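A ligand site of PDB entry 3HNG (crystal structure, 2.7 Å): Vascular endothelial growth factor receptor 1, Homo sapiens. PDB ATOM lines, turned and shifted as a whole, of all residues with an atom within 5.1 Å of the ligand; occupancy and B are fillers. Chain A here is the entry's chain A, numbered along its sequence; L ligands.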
ATOM      1  N   LEU A  35      20.553  18.366  -6.206  1.00  0.00           N
ATOM      2  CA  LEU A  35      20.922  19.736  -5.959  1.00  0.00           C
ATOM      3  C   LEU A  35      20.540  20.127  -4.553  1.00  0.00           C
ATOM      4  O   LEU A  35      20.863  21.234  -4.119  1.00  0.00           O
ATOM      5  CB  LEU A  35      20.192  20.658  -6.923  1.00  0.00           C
ATOM      6  CG  LEU A  35      20.558  20.647  -8.399  1.00  0.00           C
ATOM      7  CD1 LEU A  35      19.540  21.456  -9.177  1.00  0.00           C
ATOM      8  CD2 LEU A  35      21.919  21.210  -8.670  1.00  0.00           C
ATOM      9  N   VAL A  43      15.537  18.455  -4.675  1.00  0.00           N
ATOM     10  CA  VAL A  43      15.611  19.090  -5.973  1.00  0.00           C
ATOM     11  C   VAL A  43      16.673  18.375  -6.746  1.00  0.00           C
ATOM     12  O   VAL A  43      17.765  18.184  -6.231  1.00  0.00           O
ATOM     13  CB  VAL A  43      16.066  20.556  -5.879  1.00  0.00           C
ATOM     14  CG1 VAL A  43      16.243  21.110  -7.275  1.00  0.00           C
ATOM     15  CG2 VAL A  43      15.041  21.409  -5.077  1.00  0.00           C
ATOM     16  N   ALA A  61      15.689  22.591 -13.267  1.00  0.00           N
ATOM     17  CA  ALA A  61      15.775  22.064 -11.943  1.00  0.00           C
ATOM     18  C   ALA A  61      14.379  21.586 -11.611  1.00  0.00           C
ATOM     19  O   ALA A  61      13.386  22.242 -11.962  1.00  0.00           O
ATOM     20  CB  ALA A  61      16.201  23.132 -10.979  1.00  0.00           C
ATOM     21  N   VAL A  62      14.323  20.447 -10.936  1.00  0.00           N
ATOM     22  CA  VAL A  62      13.086  19.754 -10.665  1.00  0.00           C
ATOM     23  C   VAL A  62      12.932  19.463  -9.169  1.00  0.00           C
ATOM     24  O   VAL A  62      13.730  18.737  -8.567  1.00  0.00           O
ATOM     25  CB  VAL A  62      13.022  18.421 -11.450  1.00  0.00           C
ATOM     26  CG1 VAL A  62      11.650  17.778 -11.288  1.00  0.00           C
ATOM     27  CG2 VAL A  62      13.293  18.652 -12.879  1.00  0.00           C
ATOM     28  N   LYS A  63      11.858  19.965  -8.576  1.00  0.00           N
ATOM     29  CA  LYS A  63      11.585  19.699  -7.170  1.00  0.00           C
ATOM     30  C   LYS A  63      10.444  18.698  -7.079  1.00  0.00           C
ATOM     31  O   LYS A  63       9.501  18.745  -7.864  1.00  0.00           O
ATOM     32  CB  LYS A  63      11.317  20.993  -6.412  1.00  0.00           C
ATOM     33  CG  LYS A  63      10.397  20.841  -5.231  1.00  0.00           C
ATOM     34  CD  LYS A  63      10.738  21.726  -4.011  1.00  0.00           C
ATOM     35  CE  LYS A  63      11.328  23.110  -4.351  1.00  0.00           C
ATOM     36  NZ  LYS A  63      10.809  24.130  -3.396  1.00  0.00           N
ATOM     37  N   GLU A  80       3.092  25.235  -3.583  1.00  0.00           N
ATOM     38  CA  GLU A  80       4.194  25.970  -4.165  1.00  0.00           C
ATOM     39  C   GLU A  80       3.985  26.127  -5.673  1.00  0.00           C
ATOM     40  O   GLU A  80       4.235  27.199  -6.230  1.00  0.00           O
ATOM     41  CB  GLU A  80       5.530  25.293  -3.898  1.00  0.00           C
ATOM     42  CG  GLU A  80       6.674  26.025  -4.576  1.00  0.00           C
ATOM     43  CD  GLU A  80       8.004  25.465  -4.186  1.00  0.00           C
ATOM     44  OE1 GLU A  80       8.055  24.806  -3.109  1.00  0.00           O
ATOM     45  OE2 GLU A  80       8.985  25.621  -4.965  1.00  0.00           O
ATOM     46  N   LEU A  84       3.701  29.521  -7.901  1.00  0.00           N
ATOM     47  CA  LEU A  84       4.622  29.806  -8.998  1.00  0.00           C
ATOM     48  C   LEU A  84       3.876  30.011 -10.318  1.00  0.00           C
ATOM     49  O   LEU A  84       4.433  30.605 -11.241  1.00  0.00           O
ATOM     50  CB  LEU A  84       5.626  28.685  -9.184  1.00  0.00           C
ATOM     51  CG  LEU A  84       6.726  28.617  -8.141  1.00  0.00           C
ATOM     52  CD1 LEU A  84       7.602  27.406  -8.404  1.00  0.00           C
ATOM     53  CD2 LEU A  84       7.555  29.876  -8.166  1.00  0.00           C
ATOM     54  N   ILE A  87       2.106  33.888 -10.613  1.00  0.00           N
ATOM     55  CA  ILE A  87       3.061  34.854 -10.125  1.00  0.00           C
ATOM     56  C   ILE A  87       3.334  35.807 -11.293  1.00  0.00           C
ATOM     57  O   ILE A  87       3.024  36.988 -11.205  1.00  0.00           O
ATOM     58  CB  ILE A  87       4.345  34.154  -9.549  1.00  0.00           C
ATOM     59  CG1 ILE A  87       4.718  34.676  -8.174  1.00  0.00           C
ATOM     60  CG2 ILE A  87       5.600  34.367 -10.374  1.00  0.00           C
ATOM     61  CD1 ILE A  87       6.048  34.114  -7.733  1.00  0.00           C
ATOM     62  N   VAL A  93      13.295  36.414 -10.251  1.00  0.00           N
ATOM     63  CA  VAL A  93      12.703  35.327  -9.488  1.00  0.00           C
ATOM     64  C   VAL A  93      12.918  34.068 -10.294  1.00  0.00           C
ATOM     65  O   VAL A  93      12.891  34.134 -11.522  1.00  0.00           O
ATOM     66  CB  VAL A  93      11.191  35.526  -9.239  1.00  0.00           C
ATOM     67  CG1 VAL A  93      10.609  34.340  -8.509  1.00  0.00           C
ATOM     68  CG2 VAL A  93      10.934  36.839  -8.477  1.00  0.00           C
ATOM     69  N   VAL A  94      13.151  32.939  -9.634  1.00  0.00           N
ATOM     70  CA  VAL A  94      13.241  31.640 -10.337  1.00  0.00           C
ATOM     71  C   VAL A  94      11.934  31.345 -11.083  1.00  0.00           C
ATOM     72  O   VAL A  94      10.882  31.268 -10.477  1.00  0.00           O
ATOM     73  CB  VAL A  94      13.584  30.509  -9.369  1.00  0.00           C
ATOM     74  CG1 VAL A  94      13.171  29.176  -9.930  1.00  0.00           C
ATOM     75  CG2 VAL A  94      15.057  30.494  -9.091  1.00  0.00           C
ATOM     76  N   VAL A 109       7.799  19.885  -9.913  1.00  0.00           N
ATOM     77  CA  VAL A 109       7.793  21.280 -10.265  1.00  0.00           C
ATOM     78  C   VAL A 109       9.086  21.639 -10.991  1.00  0.00           C
ATOM     79  O   VAL A 109      10.179  21.472 -10.472  1.00  0.00           O
ATOM     80  CB  VAL A 109       7.663  22.079  -8.971  1.00  0.00           C
ATOM     81  CG1 VAL A 109       7.472  23.567  -9.251  1.00  0.00           C
ATOM     82  CG2 VAL A 109       6.520  21.532  -8.189  1.00  0.00           C
ATOM     83  N   ILE A 110       8.950  22.091 -12.220  1.00  0.00           N
ATOM     84  CA  ILE A 110      10.101  22.364 -13.052  1.00  0.00           C
ATOM     85  C   ILE A 110      10.297  23.850 -13.234  1.00  0.00           C
ATOM     86  O   ILE A 110       9.373  24.576 -13.619  1.00  0.00           O
ATOM     87  CB  ILE A 110       9.975  21.707 -14.413  1.00  0.00           C
ATOM     88  CG1 ILE A 110       9.332  20.331 -14.254  1.00  0.00           C
ATOM     89  CG2 ILE A 110      11.331  21.531 -15.036  1.00  0.00           C
ATOM     90  CD1 ILE A 110       8.977  19.686 -15.540  1.00  0.00           C
ATOM     91  N   VAL A 111      11.513  24.304 -12.923  1.00  0.00           N
ATOM     92  CA  VAL A 111      11.851  25.701 -13.016  1.00  0.00           C
ATOM     93  C   VAL A 111      13.154  25.844 -13.702  1.00  0.00           C
ATOM     94  O   VAL A 111      13.823  24.862 -14.027  1.00  0.00           O
ATOM     95  CB  VAL A 111      11.951  26.373 -11.661  1.00  0.00           C
ATOM     96  CG1 VAL A 111      10.634  26.256 -10.953  1.00  0.00           C
ATOM     97  CG2 VAL A 111      13.034  25.737 -10.842  1.00  0.00           C
ATOM     98  N   GLU A 112      13.533  27.079 -13.928  1.00  0.00           N
ATOM     99  CA  GLU A 112      14.792  27.331 -14.609  1.00  0.00           C
ATOM    100  C   GLU A 112      16.001  27.076 -13.701  1.00  0.00           C
ATOM    101  O   GLU A 112      15.970  27.271 -12.498  1.00  0.00           O
ATOM    102  CB  GLU A 112      14.831  28.759 -15.150  1.00  0.00           C
ATOM    103  CG  GLU A 112      14.714  29.800 -14.114  1.00  0.00           C
ATOM    104  CD  GLU A 112      14.589  31.174 -14.743  1.00  0.00           C
ATOM    105  OE1 GLU A 112      15.374  31.431 -15.711  1.00  0.00           O
ATOM    106  OE2 GLU A 112      13.727  31.979 -14.298  1.00  0.00           O
ATOM    107  N   TYR A 113      17.052  26.583 -14.327  1.00  0.00           N
ATOM    108  CA  TYR A 113      18.232  26.156 -13.638  1.00  0.00           C
ATOM    109  C   TYR A 113      19.192  27.299 -13.426  1.00  0.00           C
ATOM    110  O   TYR A 113      19.499  28.020 -14.369  1.00  0.00           O
ATOM    111  CB  TYR A 113      18.908  25.113 -14.507  1.00  0.00           C
ATOM    112  CG  TYR A 113      20.158  24.605 -13.868  1.00  0.00           C
ATOM    113  CD1 TYR A 113      20.156  24.211 -12.548  1.00  0.00           C
ATOM    114  CD2 TYR A 113      21.355  24.527 -14.582  1.00  0.00           C
ATOM    115  CE1 TYR A 113      21.267  23.729 -11.956  1.00  0.00           C
ATOM    116  CE2 TYR A 113      22.483  24.035 -13.987  1.00  0.00           C
ATOM    117  CZ  TYR A 113      22.438  23.641 -12.679  1.00  0.00           C
ATOM    118  OH  TYR A 113      23.545  23.167 -12.046  1.00  0.00           O
ATOM    119  N   CYS A 114      19.698  27.461 -12.204  1.00  0.00           N
ATOM    120  CA  CYS A 114      20.685  28.518 -11.967  1.00  0.00           C
ATOM    121  C   CYS A 114      22.066  27.940 -11.757  1.00  0.00           C
ATOM    122  O   CYS A 114      22.351  27.420 -10.710  1.00  0.00           O
ATOM    123  CB  CYS A 114      20.297  29.328 -10.745  1.00  0.00           C
ATOM    124  SG  CYS A 114      18.689  30.053 -10.976  1.00  0.00           S
ATOM    125  N   LEU A 215       7.301  40.218  -5.863  1.00  0.00           N
ATOM    126  CA  LEU A 215       6.640  39.234  -4.996  1.00  0.00           C
ATOM    127  C   LEU A 215       5.643  39.886  -4.083  1.00  0.00           C
ATOM    128  O   LEU A 215       4.513  39.452  -4.020  1.00  0.00           O
ATOM    129  CB  LEU A 215       7.643  38.416  -4.168  1.00  0.00           C
ATOM    130  CG  LEU A 215       8.561  37.493  -4.983  1.00  0.00           C
ATOM    131  CD1 LEU A 215       9.312  36.541  -4.092  1.00  0.00           C
ATOM    132  CD2 LEU A 215       7.801  36.705  -5.996  1.00  0.00           C
ATOM    133  N   CYS A 220       2.726  38.126  -1.880  1.00  0.00           N
ATOM    134  CA  CYS A 220       3.456  36.970  -1.560  1.00  0.00           C
ATOM    135  C   CYS A 220       4.600  37.278  -0.609  1.00  0.00           C
ATOM    136  O   CYS A 220       5.500  38.050  -0.901  1.00  0.00           O
ATOM    137  CB  CYS A 220       3.921  36.312  -2.853  1.00  0.00           C
ATOM    138  SG  CYS A 220       5.189  35.087  -2.617  1.00  0.00           S
ATOM    139  N   HIS A 222       7.721  35.904   1.549  1.00  0.00           N
ATOM    140  CA  HIS A 222       8.709  34.848   1.278  1.00  0.00           C
ATOM    141  C   HIS A 222       9.013  33.981   2.483  1.00  0.00           C
ATOM    142  O   HIS A 222       9.055  32.761   2.403  1.00  0.00           O
ATOM    143  CB  HIS A 222      10.002  35.458   0.789  1.00  0.00           C
ATOM    144  CG  HIS A 222      10.955  34.446   0.239  1.00  0.00           C
ATOM    145  ND1 HIS A 222      11.684  33.588   1.046  1.00  0.00           N
ATOM    146  CD2 HIS A 222      11.279  34.121  -1.041  1.00  0.00           C
ATOM    147  CE1 HIS A 222      12.400  32.781   0.283  1.00  0.00           C
ATOM    148  NE2 HIS A 222      12.179  33.090  -0.980  1.00  0.00           N
ATOM    149  N   LEU A 231      19.962  32.795  -5.907  1.00  0.00           N
ATOM    150  CA  LEU A 231      20.697  31.953  -6.799  1.00  0.00           C
ATOM    151  C   LEU A 231      21.209  32.763  -7.990  1.00  0.00           C
ATOM    152  O   LEU A 231      20.555  33.708  -8.465  1.00  0.00           O
ATOM    153  CB  LEU A 231      19.788  30.847  -7.272  1.00  0.00           C
ATOM    154  CG  LEU A 231      19.829  29.473  -6.573  1.00  0.00           C
ATOM    155  CD1 LEU A 231      19.849  29.531  -5.087  1.00  0.00           C
ATOM    156  CD2 LEU A 231      18.627  28.641  -7.024  1.00  0.00           C
ATOM    157  N   ILE A 240      15.738  35.054  -6.959  1.00  0.00           N
ATOM    158  CA  ILE A 240      15.098  34.571  -5.725  1.00  0.00           C
ATOM    159  C   ILE A 240      14.457  33.191  -5.868  1.00  0.00           C
ATOM    160  O   ILE A 240      13.632  32.920  -6.735  1.00  0.00           O
ATOM    161  CB  ILE A 240      13.997  35.506  -5.292  1.00  0.00           C
ATOM    162  CG1 ILE A 240      14.555  36.896  -5.058  1.00  0.00           C
ATOM    163  CG2 ILE A 240      13.364  34.965  -4.025  1.00  0.00           C
ATOM    164  CD1 ILE A 240      13.485  37.973  -5.016  1.00  0.00           C
ATOM    165  N   CYS A 241      14.848  32.301  -4.982  1.00  0.00           N
ATOM    166  CA  CYS A 241      14.308  30.985  -4.989  1.00  0.00           C
ATOM    167  C   CYS A 241      13.890  30.634  -3.561  1.00  0.00           C
ATOM    168  O   CYS A 241      14.059  31.476  -2.647  1.00  0.00           O
ATOM    169  CB  CYS A 241      15.364  30.015  -5.521  1.00  0.00           C
ATOM    170  SG  CYS A 241      16.568  29.525  -4.269  1.00  0.00           S
ATOM    171  N   ASP A 242      13.341  29.426  -3.400  1.00  0.00           N
ATOM    172  CA  ASP A 242      13.065  28.816  -2.070  1.00  0.00           C
ATOM    173  C   ASP A 242      13.147  27.280  -2.247  1.00  0.00           C
ATOM    174  O   ASP A 242      12.351  26.707  -2.949  1.00  0.00           O
ATOM    175  CB  ASP A 242      11.694  29.273  -1.514  1.00  0.00           C
ATOM    176  CG  ASP A 242      11.433  28.790  -0.082  1.00  0.00           C
ATOM    177  OD1 ASP A 242      10.362  29.108   0.501  1.00  0.00           O
ATOM    178  OD2 ASP A 242      12.287  28.094   0.493  1.00  0.00           O
ATOM    179  N   PHE A 243      14.139  26.630  -1.646  1.00  0.00           N
ATOM    180  CA  PHE A 243      14.297  25.189  -1.760  1.00  0.00           C
ATOM    181  C   PHE A 243      13.176  24.475  -1.033  1.00  0.00           C
ATOM    182  O   PHE A 243      12.730  23.385  -1.446  1.00  0.00           O
ATOM    183  CB  PHE A 243      15.617  24.752  -1.155  1.00  0.00           C
ATOM    184  CG  PHE A 243      16.772  24.828  -2.097  1.00  0.00           C
ATOM    185  CD1 PHE A 243      17.175  23.707  -2.814  1.00  0.00           C
ATOM    186  CD2 PHE A 243      17.486  25.995  -2.269  1.00  0.00           C
ATOM    187  CE1 PHE A 243      18.251  23.757  -3.672  1.00  0.00           C
ATOM    188  CE2 PHE A 243      18.559  26.055  -3.136  1.00  0.00           C
ATOM    189  CZ  PHE A 243      18.940  24.924  -3.833  1.00  0.00           C
HETATM  190 CL1  LIG L   1       9.156  33.023  -4.161  1.00  0.00          CL
HETATM  191  C1  LIG L   1       9.520  31.375  -4.658  1.00  0.00           C
HETATM  192  C2  LIG L   1       8.919  30.314  -4.002  1.00  0.00           C
HETATM  193  C3  LIG L   1       9.312  28.996  -4.418  1.00  0.00           C
HETATM  194  C4  LIG L   1      10.537  31.248  -5.765  1.00  0.00           C
HETATM  195  C5  LIG L   1      10.858  29.964  -6.187  1.00  0.00           C
HETATM  196  C6  LIG L   1      10.384  28.885  -5.407  1.00  0.00           C
HETATM  197  N1  LIG L   1      10.685  27.605  -5.954  1.00  0.00           N
HETATM  198  C7  LIG L   1      12.072  27.234  -6.120  1.00  0.00           C
HETATM  199  O1  LIG L   1      12.937  27.975  -5.810  1.00  0.00           O
HETATM  200  C8  LIG L   1      12.247  25.847  -6.741  1.00  0.00           C
HETATM  201  C9  LIG L   1      13.478  25.221  -6.905  1.00  0.00           C
HETATM  202  C10 LIG L   1      13.647  24.031  -7.692  1.00  0.00           C
HETATM  203  C11 LIG L   1      12.478  23.448  -8.308  1.00  0.00           C
HETATM  204  C12 LIG L   1      11.198  24.112  -8.198  1.00  0.00           C
HETATM  205  C13 LIG L   1      11.073  25.304  -7.451  1.00  0.00           C
HETATM  206  N2  LIG L   1      14.708  25.704  -6.410  1.00  0.00           N
HETATM  207  C14 LIG L   1      16.138  25.517  -6.279  1.00  0.00           C
HETATM  208  C15 LIG L   1      16.854  25.594  -7.635  1.00  0.00           C
HETATM  209  C16 LIG L   1      18.118  25.143  -7.763  1.00  0.00           C
HETATM  210  C17 LIG L   1      18.796  25.340  -8.999  1.00  0.00           C
HETATM  211  N3  LIG L   1      18.265  26.246  -9.953  1.00  0.00           N
HETATM  212  C18 LIG L   1      16.978  26.773  -9.791  1.00  0.00           C
HETATM  213  C19 LIG L   1      16.321  26.559  -8.592  1.00  0.00           C
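A nitrogen (N1) of the ligand lies within hydrogen-bond range of the side-chain carboxylate of Glu 80 (2.8 Å). An oxygen (O1) of the ligand sits at hydrogen-bond distance from the backbone NH (N) of Asp 242 (2.8 Å). The backbone NH (N) of Cys 114 is in hydrogen-bond range of a nitrogen (N3) of the ligand (2.9 Å).
Leu 35 touches the ligand (CD1 to C17, 3.96 Å). CG1 of Val 43 touches C10 of the ligand (3.9 Å). Ala 61 touches the ligand (CB to N3, 3.9 Å). Lys 63 touches the ligand (CB to C11, 3.3 Å). Leu 84 touches the ligand (CD2 to C5, 3.9 Å). O of Val 109 touches C12 of the ligand, 3.6 Å away. Val 111 touches the ligand. Glu 112 touches the ligand. CA of Tyr 113 touches N3 of the ligand, 3.7 Å away. Leu 215 touches the ligand. His 222 touches the ligand. CD2 of Leu 231 touches C19 of the ligand, at 3.5 Å. Ile 240 touches the ligand. Cys 241 touches the ligand (CB to O1, 3.2 Å). Phe 243 touches the ligand (CZ to C14, 3.8 Å). Hydrophobic or aromatic side chains within 4 Å of the ligand: Leu 35, Val 43, Ala 61, Leu 84, Val 109, Val 111, Tyr 113, Leu 215, His 222, Leu 231 and Phe 243. Of the 24 residues printed, 18 come within 4 Å of the ligand. Along chain A the residues within 4 Å of the ligand span positions 35 to 243.
The side-chain amino group (NZ) of Lys 63 is in salt-bridge range of the side-chain carboxylate (OE2) of Glu 80. The side-chain amino group of Lys 63 lies within hydrogen-bond range of the backbone carbonyl oxygen of Asp 242 (3.0 Å). O of Cys 241 is in hydrogen-bond range of NE2 of His 222 (3.0 Å). The backbone carbonyl oxygen of Lys 63 lies within hydrogen-bond range of the backbone NH of Val 109 (2.9 Å). The side-chain amino group of Lys 63 lies within hydrogen-bond range of the backbone carbonyl oxygen of Phe 243. The backbone carbonyl oxygen (O) of Leu 215 is in hydrogen-bond range of the backbone NH (N) of Cys 220 (3.1 Å). The backbone NH of Val 94 lies within hydrogen-bond range of the backbone carbonyl oxygen of Ile 240 (2.9 Å). The backbone carbonyl oxygen of Val 43 is in hydrogen-bond range of the backbone NH of Leu 35 (2.8 Å).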
